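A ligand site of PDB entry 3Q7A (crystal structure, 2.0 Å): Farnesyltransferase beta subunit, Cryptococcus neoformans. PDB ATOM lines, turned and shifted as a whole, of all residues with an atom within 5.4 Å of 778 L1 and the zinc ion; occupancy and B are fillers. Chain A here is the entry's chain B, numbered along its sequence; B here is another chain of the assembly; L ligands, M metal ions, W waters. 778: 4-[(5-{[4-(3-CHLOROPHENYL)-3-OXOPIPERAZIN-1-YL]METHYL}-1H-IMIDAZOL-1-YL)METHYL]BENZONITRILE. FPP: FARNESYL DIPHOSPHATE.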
ATOM      1  N   LEU A  84     -27.233  23.466  28.202  1.00  0.00           N
ATOM      2  CA  LEU A  84     -26.753  22.901  29.461  1.00  0.00           C
ATOM      3  C   LEU A  84     -27.515  23.426  30.685  1.00  0.00           C
ATOM      4  O   LEU A  84     -27.028  23.327  31.819  1.00  0.00           O
ATOM      5  CB  LEU A  84     -25.239  23.144  29.625  1.00  0.00           C
ATOM      6  CG  LEU A  84     -24.300  22.461  28.629  1.00  0.00           C
ATOM      7  CD1 LEU A  84     -22.899  23.043  28.730  1.00  0.00           C
ATOM      8  CD2 LEU A  84     -24.286  20.951  28.835  1.00  0.00           C
ATOM      9  N   SER A  87     -27.910  21.053  33.308  1.00  0.00           N
ATOM     10  CA  SER A  87     -26.601  20.577  33.749  1.00  0.00           C
ATOM     11  C   SER A  87     -25.766  21.634  34.479  1.00  0.00           C
ATOM     12  O   SER A  87     -24.541  21.520  34.544  1.00  0.00           O
ATOM     13  CB  SER A  87     -25.805  20.028  32.559  1.00  0.00           C
ATOM     14  OG  SER A  87     -26.373  18.824  32.091  1.00  0.00           O
ATOM     15  N   TRP A  90     -23.093  20.660  36.952  1.00  0.00           N
ATOM     16  CA  TRP A  90     -21.880  20.167  36.293  1.00  0.00           C
ATOM     17  C   TRP A  90     -20.959  21.309  35.904  1.00  0.00           C
ATOM     18  O   TRP A  90     -19.746  21.205  36.053  1.00  0.00           O
ATOM     19  CB  TRP A  90     -22.220  19.313  35.068  1.00  0.00           C
ATOM     20  CG  TRP A  90     -22.714  17.938  35.417  1.00  0.00           C
ATOM     21  CD1 TRP A  90     -23.999  17.489  35.334  1.00  0.00           C
ATOM     22  CD2 TRP A  90     -21.928  16.843  35.908  1.00  0.00           C
ATOM     23  NE1 TRP A  90     -24.059  16.172  35.742  1.00  0.00           N
ATOM     24  CE2 TRP A  90     -22.812  15.759  36.102  1.00  0.00           C
ATOM     25  CE3 TRP A  90     -20.564  16.670  36.207  1.00  0.00           C
ATOM     26  CZ2 TRP A  90     -22.367  14.515  36.580  1.00  0.00           C
ATOM     27  CZ3 TRP A  90     -20.134  15.443  36.681  1.00  0.00           C
ATOM     28  CH2 TRP A  90     -21.039  14.373  36.861  1.00  0.00           C
ATOM     29  N   TRP A  94     -17.302  21.241  37.229  1.00  0.00           N
ATOM     30  CA  TRP A  94     -16.191  21.325  36.285  1.00  0.00           C
ATOM     31  C   TRP A  94     -15.266  22.495  36.601  1.00  0.00           C
ATOM     32  O   TRP A  94     -14.053  22.372  36.514  1.00  0.00           O
ATOM     33  CB  TRP A  94     -16.674  21.405  34.825  1.00  0.00           C
ATOM     34  CG  TRP A  94     -17.403  20.165  34.331  1.00  0.00           C
ATOM     35  CD1 TRP A  94     -17.133  18.862  34.658  1.00  0.00           C
ATOM     36  CD2 TRP A  94     -18.500  20.137  33.414  1.00  0.00           C
ATOM     37  NE1 TRP A  94     -18.007  18.018  34.006  1.00  0.00           N
ATOM     38  CE2 TRP A  94     -18.853  18.777  33.233  1.00  0.00           C
ATOM     39  CE3 TRP A  94     -19.223  21.120  32.731  1.00  0.00           C
ATOM     40  CZ2 TRP A  94     -19.908  18.382  32.394  1.00  0.00           C
ATOM     41  CZ3 TRP A  94     -20.264  20.725  31.892  1.00  0.00           C
ATOM     42  CH2 TRP A  94     -20.596  19.363  31.734  1.00  0.00           C
ATOM     43  N   LEU A 141     -27.476  12.534  38.768  1.00  0.00           N
ATOM     44  CA  LEU A 141     -26.227  13.109  38.259  1.00  0.00           C
ATOM     45  C   LEU A 141     -25.882  14.501  38.831  1.00  0.00           C
ATOM     46  O   LEU A 141     -24.766  14.700  39.307  1.00  0.00           O
ATOM     47  CB  LEU A 141     -26.185  13.075  36.724  1.00  0.00           C
ATOM     48  CG  LEU A 141     -25.734  11.760  36.065  1.00  0.00           C
ATOM     49  CD1 LEU A 141     -26.550  10.535  36.517  1.00  0.00           C
ATOM     50  CD2 LEU A 141     -25.761  11.866  34.546  1.00  0.00           C
ATOM     51  N   ARG A 197     -24.176   5.308  35.019  1.00  0.00           N
ATOM     52  CA  ARG A 197     -23.925   6.685  35.488  1.00  0.00           C
ATOM     53  C   ARG A 197     -24.738   6.968  36.740  1.00  0.00           C
ATOM     54  O   ARG A 197     -24.241   7.546  37.701  1.00  0.00           O
ATOM     55  CB  ARG A 197     -24.281   7.726  34.419  1.00  0.00           C
ATOM     56  CG  ARG A 197     -23.507   7.657  33.108  1.00  0.00           C
ATOM     57  CD  ARG A 197     -24.139   8.591  32.074  1.00  0.00           C
ATOM     58  NE  ARG A 197     -25.585   8.356  31.962  1.00  0.00           N
ATOM     59  CZ  ARG A 197     -26.495   9.270  31.632  1.00  0.00           C
ATOM     60  NH1 ARG A 197     -26.135  10.512  31.354  1.00  0.00           N
ATOM     61  NH2 ARG A 197     -27.778   8.929  31.572  1.00  0.00           N
ATOM     62  N   ASP A 323      -9.479  11.218  22.681  1.00  0.00           N
ATOM     63  CA  ASP A 323     -10.194  12.379  23.192  1.00  0.00           C
ATOM     64  C   ASP A 323      -9.698  12.672  24.601  1.00  0.00           C
ATOM     65  O   ASP A 323      -9.681  11.781  25.454  1.00  0.00           O
ATOM     66  CB  ASP A 323     -11.701  12.120  23.179  1.00  0.00           C
ATOM     67  CG  ASP A 323     -12.532  13.258  23.752  1.00  0.00           C
ATOM     68  OD1 ASP A 323     -12.010  14.128  24.483  1.00  0.00           O
ATOM     69  OD2 ASP A 323     -13.750  13.286  23.471  1.00  0.00           O
ATOM     70  N   GLY A 324      -9.302  13.915  24.824  1.00  0.00           N
ATOM     71  CA  GLY A 324      -8.768  14.367  26.104  1.00  0.00           C
ATOM     72  C   GLY A 324      -9.590  14.035  27.335  1.00  0.00           C
ATOM     73  O   GLY A 324      -9.031  13.803  28.411  1.00  0.00           O
ATOM     74  N   CYS A 325     -10.914  14.023  27.210  1.00  0.00           N
ATOM     75  CA  CYS A 325     -11.763  13.753  28.383  1.00  0.00           C
ATOM     76  C   CYS A 325     -11.606  12.328  28.913  1.00  0.00           C
ATOM     77  O   CYS A 325     -11.819  12.087  30.102  1.00  0.00           O
ATOM     78  CB  CYS A 325     -13.240  14.098  28.126  1.00  0.00           C
ATOM     79  SG  CYS A 325     -14.122  13.029  26.958  1.00  0.00           S
ATOM     80  N   TYR A 326     -11.212  11.393  28.045  1.00  0.00           N
ATOM     81  CA  TYR A 326     -11.020   9.993  28.441  1.00  0.00           C
ATOM     82  C   TYR A 326      -9.746   9.760  29.250  1.00  0.00           C
ATOM     83  O   TYR A 326      -9.512   8.652  29.735  1.00  0.00           O
ATOM     84  CB  TYR A 326     -11.110   9.059  27.228  1.00  0.00           C
ATOM     85  CG  TYR A 326     -12.459   9.150  26.557  1.00  0.00           C
ATOM     86  CD1 TYR A 326     -13.633   8.977  27.282  1.00  0.00           C
ATOM     87  CD2 TYR A 326     -12.557   9.438  25.199  1.00  0.00           C
ATOM     88  CE1 TYR A 326     -14.879   9.092  26.684  1.00  0.00           C
ATOM     89  CE2 TYR A 326     -13.802   9.545  24.586  1.00  0.00           C
ATOM     90  CZ  TYR A 326     -14.957   9.369  25.333  1.00  0.00           C
ATOM     91  OH  TYR A 326     -16.189   9.467  24.738  1.00  0.00           O
ATOM     92  N   TRP A 329     -11.812   9.394  32.285  1.00  0.00           N
ATOM     93  CA  TRP A 329     -12.725   8.245  32.264  1.00  0.00           C
ATOM     94  C   TRP A 329     -12.010   6.905  32.122  1.00  0.00           C
ATOM     95  O   TRP A 329     -12.325   5.953  32.840  1.00  0.00           O
ATOM     96  CB  TRP A 329     -13.827   8.397  31.204  1.00  0.00           C
ATOM     97  CG  TRP A 329     -14.625   9.666  31.350  1.00  0.00           C
ATOM     98  CD1 TRP A 329     -14.679  10.692  30.465  1.00  0.00           C
ATOM     99  CD2 TRP A 329     -15.441  10.042  32.470  1.00  0.00           C
ATOM    100  NE1 TRP A 329     -15.494  11.695  30.945  1.00  0.00           N
ATOM    101  CE2 TRP A 329     -15.974  11.324  32.168  1.00  0.00           C
ATOM    102  CE3 TRP A 329     -15.785   9.428  33.683  1.00  0.00           C
ATOM    103  CZ2 TRP A 329     -16.829  12.000  33.051  1.00  0.00           C
ATOM    104  CZ3 TRP A 329     -16.633  10.115  34.560  1.00  0.00           C
ATOM    105  CH2 TRP A 329     -17.143  11.388  34.232  1.00  0.00           C
ATOM    106  N   ASP A 400     -11.139  18.405  23.627  1.00  0.00           N
ATOM    107  CA  ASP A 400     -11.217  17.054  23.099  1.00  0.00           C
ATOM    108  C   ASP A 400      -9.932  16.705  22.328  1.00  0.00           C
ATOM    109  O   ASP A 400      -9.189  15.806  22.717  1.00  0.00           O
ATOM    110  CB  ASP A 400     -12.470  16.972  22.204  1.00  0.00           C
ATOM    111  CG  ASP A 400     -12.526  15.743  21.311  1.00  0.00           C
ATOM    112  OD1 ASP A 400     -11.615  14.878  21.338  1.00  0.00           O
ATOM    113  OD2 ASP A 400     -13.510  15.658  20.560  1.00  0.00           O
ATOM    114  N   TYR A 409     -16.273  21.029  30.493  1.00  0.00           N
ATOM    115  CA  TYR A 409     -16.263  19.571  30.614  1.00  0.00           C
ATOM    116  C   TYR A 409     -14.894  18.975  30.259  1.00  0.00           C
ATOM    117  O   TYR A 409     -14.357  18.160  31.013  1.00  0.00           O
ATOM    118  CB  TYR A 409     -17.373  18.955  29.747  1.00  0.00           C
ATOM    119  CG  TYR A 409     -17.222  17.471  29.496  1.00  0.00           C
ATOM    120  CD1 TYR A 409     -17.621  16.531  30.455  1.00  0.00           C
ATOM    121  CD2 TYR A 409     -16.669  17.004  28.306  1.00  0.00           C
ATOM    122  CE1 TYR A 409     -17.475  15.161  30.230  1.00  0.00           C
ATOM    123  CE2 TYR A 409     -16.508  15.638  28.073  1.00  0.00           C
ATOM    124  CZ  TYR A 409     -16.915  14.735  29.039  1.00  0.00           C
ATOM    125  OH  TYR A 409     -16.755  13.386  28.805  1.00  0.00           O
ATOM    126  N   HIS A 410     -14.322  19.397  29.133  1.00  0.00           N
ATOM    127  CA  HIS A 410     -13.010  18.894  28.746  1.00  0.00           C
ATOM    128  C   HIS A 410     -11.876  19.450  29.594  1.00  0.00           C
ATOM    129  O   HIS A 410     -10.882  18.770  29.825  1.00  0.00           O
ATOM    130  CB  HIS A 410     -12.758  19.102  27.245  1.00  0.00           C
ATOM    131  CG  HIS A 410     -13.475  18.119  26.390  1.00  0.00           C
ATOM    132  ND1 HIS A 410     -14.700  18.399  25.813  1.00  0.00           N
ATOM    133  CD2 HIS A 410     -13.177  16.846  26.042  1.00  0.00           C
ATOM    134  CE1 HIS A 410     -15.105  17.335  25.130  1.00  0.00           C
ATOM    135  NE2 HIS A 410     -14.204  16.389  25.262  1.00  0.00           N
ATOM    136  N   TYR B 123     -30.033  11.966  25.566  1.00  0.00           N
ATOM    137  CA  TYR B 123     -30.472  10.811  26.352  1.00  0.00           C
ATOM    138  C   TYR B 123     -32.002  10.808  26.474  1.00  0.00           C
ATOM    139  O   TYR B 123     -32.644   9.754  26.366  1.00  0.00           O
ATOM    140  CB  TYR B 123     -29.892  10.874  27.767  1.00  0.00           C
ATOM    141  CG  TYR B 123     -28.488  10.334  27.930  1.00  0.00           C
ATOM    142  CD1 TYR B 123     -28.262   8.980  28.182  1.00  0.00           C
ATOM    143  CD2 TYR B 123     -27.384  11.184  27.856  1.00  0.00           C
ATOM    144  CE1 TYR B 123     -26.966   8.478  28.338  1.00  0.00           C
ATOM    145  CE2 TYR B 123     -26.088  10.694  28.019  1.00  0.00           C
ATOM    146  CZ  TYR B 123     -25.890   9.344  28.261  1.00  0.00           C
ATOM    147  OH  TYR B 123     -24.608   8.853  28.422  1.00  0.00           O
HETATM  148  N1  778 L   1     -20.657  15.155  25.677  1.00  0.00           N
HETATM  149  C2  778 L   1     -20.118  16.397  26.266  1.00  0.00           C
HETATM  150  C3  778 L   1     -20.096  14.919  24.338  1.00  0.00           C
HETATM  151  C4  778 L   1     -22.127  15.210  25.696  1.00  0.00           C
HETATM  152  C5  778 L   1     -20.327  16.362  27.792  1.00  0.00           C
HETATM  153  C7  778 L   1     -18.691  14.306  24.518  1.00  0.00           C
HETATM  154  C8  778 L   1     -22.578  15.336  27.162  1.00  0.00           C
HETATM  155  N9  778 L   1     -21.713  15.896  28.138  1.00  0.00           N
HETATM  156  N11 778 L   1     -18.389  13.039  24.751  1.00  0.00           N
HETATM  157  C12 778 L   1     -17.541  14.971  24.496  1.00  0.00           C
HETATM  158  O13 778 L   1     -23.696  14.949  27.481  1.00  0.00           O
HETATM  159  C14 778 L   1     -22.115  15.987  29.497  1.00  0.00           C
HETATM  160  C16 778 L   1     -19.344  11.921  24.835  1.00  0.00           C
HETATM  161  C17 778 L   1     -17.072  12.886  24.855  1.00  0.00           C
HETATM  162  N18 778 L   1     -16.542  14.108  24.709  1.00  0.00           N
HETATM  163  C20 778 L   1     -21.434  15.222  30.442  1.00  0.00           C
HETATM  164  C21 778 L   1     -23.154  16.818  29.899  1.00  0.00           C
HETATM  165  C25 778 L   1     -20.199  11.925  26.108  1.00  0.00           C
HETATM  166  C26 778 L   1     -21.799  15.283  31.786  1.00  0.00           C
HETATM  167  C27 778 L   1     -23.526  16.884  31.246  1.00  0.00           C
HETATM  168  C28 778 L   1     -21.543  11.544  26.013  1.00  0.00           C
HETATM  169  C29 778 L   1     -19.660  12.273  27.344  1.00  0.00           C
HETATM  170  C30 778 L   1     -22.845  16.103  32.194  1.00  0.00           C
HETATM  171 CL31 778 L   1     -20.925  14.328  32.932  1.00  0.00          CL
HETATM  172  C32 778 L   1     -22.347  11.531  27.143  1.00  0.00           C
HETATM  173  C33 778 L   1     -20.472  12.249  28.479  1.00  0.00           C
HETATM  174  C34 778 L   1     -21.808  11.878  28.379  1.00  0.00           C
HETATM  175  C35 778 L   1     -22.636  11.852  29.546  1.00  0.00           C
HETATM  176  N36 778 L   1     -23.295  11.847  30.482  1.00  0.00           N
HETATM  177  C1  FPP L   2     -20.651   8.197  23.475  1.00  0.00           C
HETATM  178  O1  FPP L   2     -20.566   9.538  22.979  1.00  0.00           O
HETATM  179  C2  FPP L   2     -20.648   8.186  24.874  1.00  0.00           C
HETATM  180  C3  FPP L   2     -21.724   7.994  25.752  1.00  0.00           C
HETATM  181  C4  FPP L   2     -23.141   7.774  25.207  1.00  0.00           C
HETATM  182  C5  FPP L   2     -21.545   7.987  27.284  1.00  0.00           C
HETATM  183  C6  FPP L   2     -20.231   8.613  27.791  1.00  0.00           C
HETATM  184  C7  FPP L   2     -20.165   8.615  29.188  1.00  0.00           C
HETATM  185  C8  FPP L   2     -19.222   9.249  30.003  1.00  0.00           C
HETATM  186  C10 FPP L   2     -18.029  10.007  29.386  1.00  0.00           C
HETATM  187  C9  FPP L   2     -19.251   9.108  31.524  1.00  0.00           C
HETATM  188  C11 FPP L   2     -20.462   9.712  32.230  1.00  0.00           C
HETATM  189  C12 FPP L   2     -20.218   9.727  33.607  1.00  0.00           C
HETATM  190  C13 FPP L   2     -20.917  10.426  34.598  1.00  0.00           C
HETATM  191  C14 FPP L   2     -22.114  11.300  34.236  1.00  0.00           C
HETATM  192  C15 FPP L   2     -20.481  10.305  36.057  1.00  0.00           C
HETATM  193  PA  FPP L   2     -19.822   9.922  21.579  1.00  0.00           P
HETATM  194  O1A FPP L   2     -20.139   8.924  20.538  1.00  0.00           O
HETATM  195  O2A FPP L   2     -20.122  11.345  21.339  1.00  0.00           O
HETATM  196  O3A FPP L   2     -18.262   9.815  22.001  1.00  0.00           O
HETATM  197  PB  FPP L   2     -17.191   8.734  21.410  1.00  0.00           P
HETATM  198  O1B FPP L   2     -16.988   8.846  19.948  1.00  0.00           O
HETATM  199  O2B FPP L   2     -17.659   7.278  21.853  1.00  0.00           O
HETATM  200  O3B FPP L   2     -15.864   9.031  22.252  1.00  0.00           O
HETATM  201 ZN    ZN M   1     -14.496  14.377  25.111  1.00  0.00          ZN
HETATM  202  O   HOH W   1     -17.876  13.023  21.295  1.00  0.00           O
HETATM  203  O   HOH W   2     -26.066  15.002  29.221  1.00  0.00           O
HETATM  204  O   HOH W   3     -25.382  13.841  25.752  1.00  0.00           O
HETATM  205  O   HOH W   4     -17.972  18.713  25.097  1.00  0.00           O
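N36 of 778 L1 lies within hydrogen-bond range of NH1 of Arg 197. O3B of FPP L2 sits at hydrogen-bond distance from OH of Tyr 326 (2.5 Å).
Tyr 409 touches the zinc ion. Of the 15 residues printed, 4 come within 4 Å of the zinc ion.
OG of Ser 87 touches C27 of 778 L1, 3.5 Å away. CD1 of Trp 90 touches C30 of 778 L1, at 3.6 Å. CZ2 of Trp 94 touches C26 of 778 L1 (3.7 Å). Tyr 326 touches 778 L1 (OH to C17, 3.5 Å). OH of Tyr 409 touches C29 of 778 L1, 3.4 Å away. Tyr 123 of chain B touches 778 L1 (OH to C32, 3.7 Å). Hydrophobic or aromatic side chains within 4 Å of 778 L1: Trp 90, Trp 94, Tyr 409, His 410 and Tyr 123 of chain B. Within 4 Å of 778 L1: Ser 87, Trp 90, Trp 94, Arg 197, Asp 323, Cys 325, Tyr 326, Tyr 409, His 410 and Tyr 123 of chain B. Along chain A the residues within 4 Å of 778 L1 span positions 87 to 410. The nearest printed residue that does not touch 778 L1 is Leu 84 (4.4 Å).
OH of Tyr 409 sits close to SG of Cys 325, at 3.2 Å. The indole nitrogen (NE1) of Trp 329 lies within hydrogen-bond range of the side-chain hydroxyl (OH) of Tyr 409.
The zinc ion is bound by a ring nitrogen (NE2) of His 410 (2.0 Å), a nitrogen (N18) of 778 L1 (2.1 Å), the side-chain carboxylate (OD2) of Asp 323 (2.1 Å), the side-chain sulfur (SG) of Cys 325 (2.3 Å) and the side-chain carboxylate (OD1) of Asp 323 (2.6 Å). The zinc ion has five donor atoms within binding distance.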
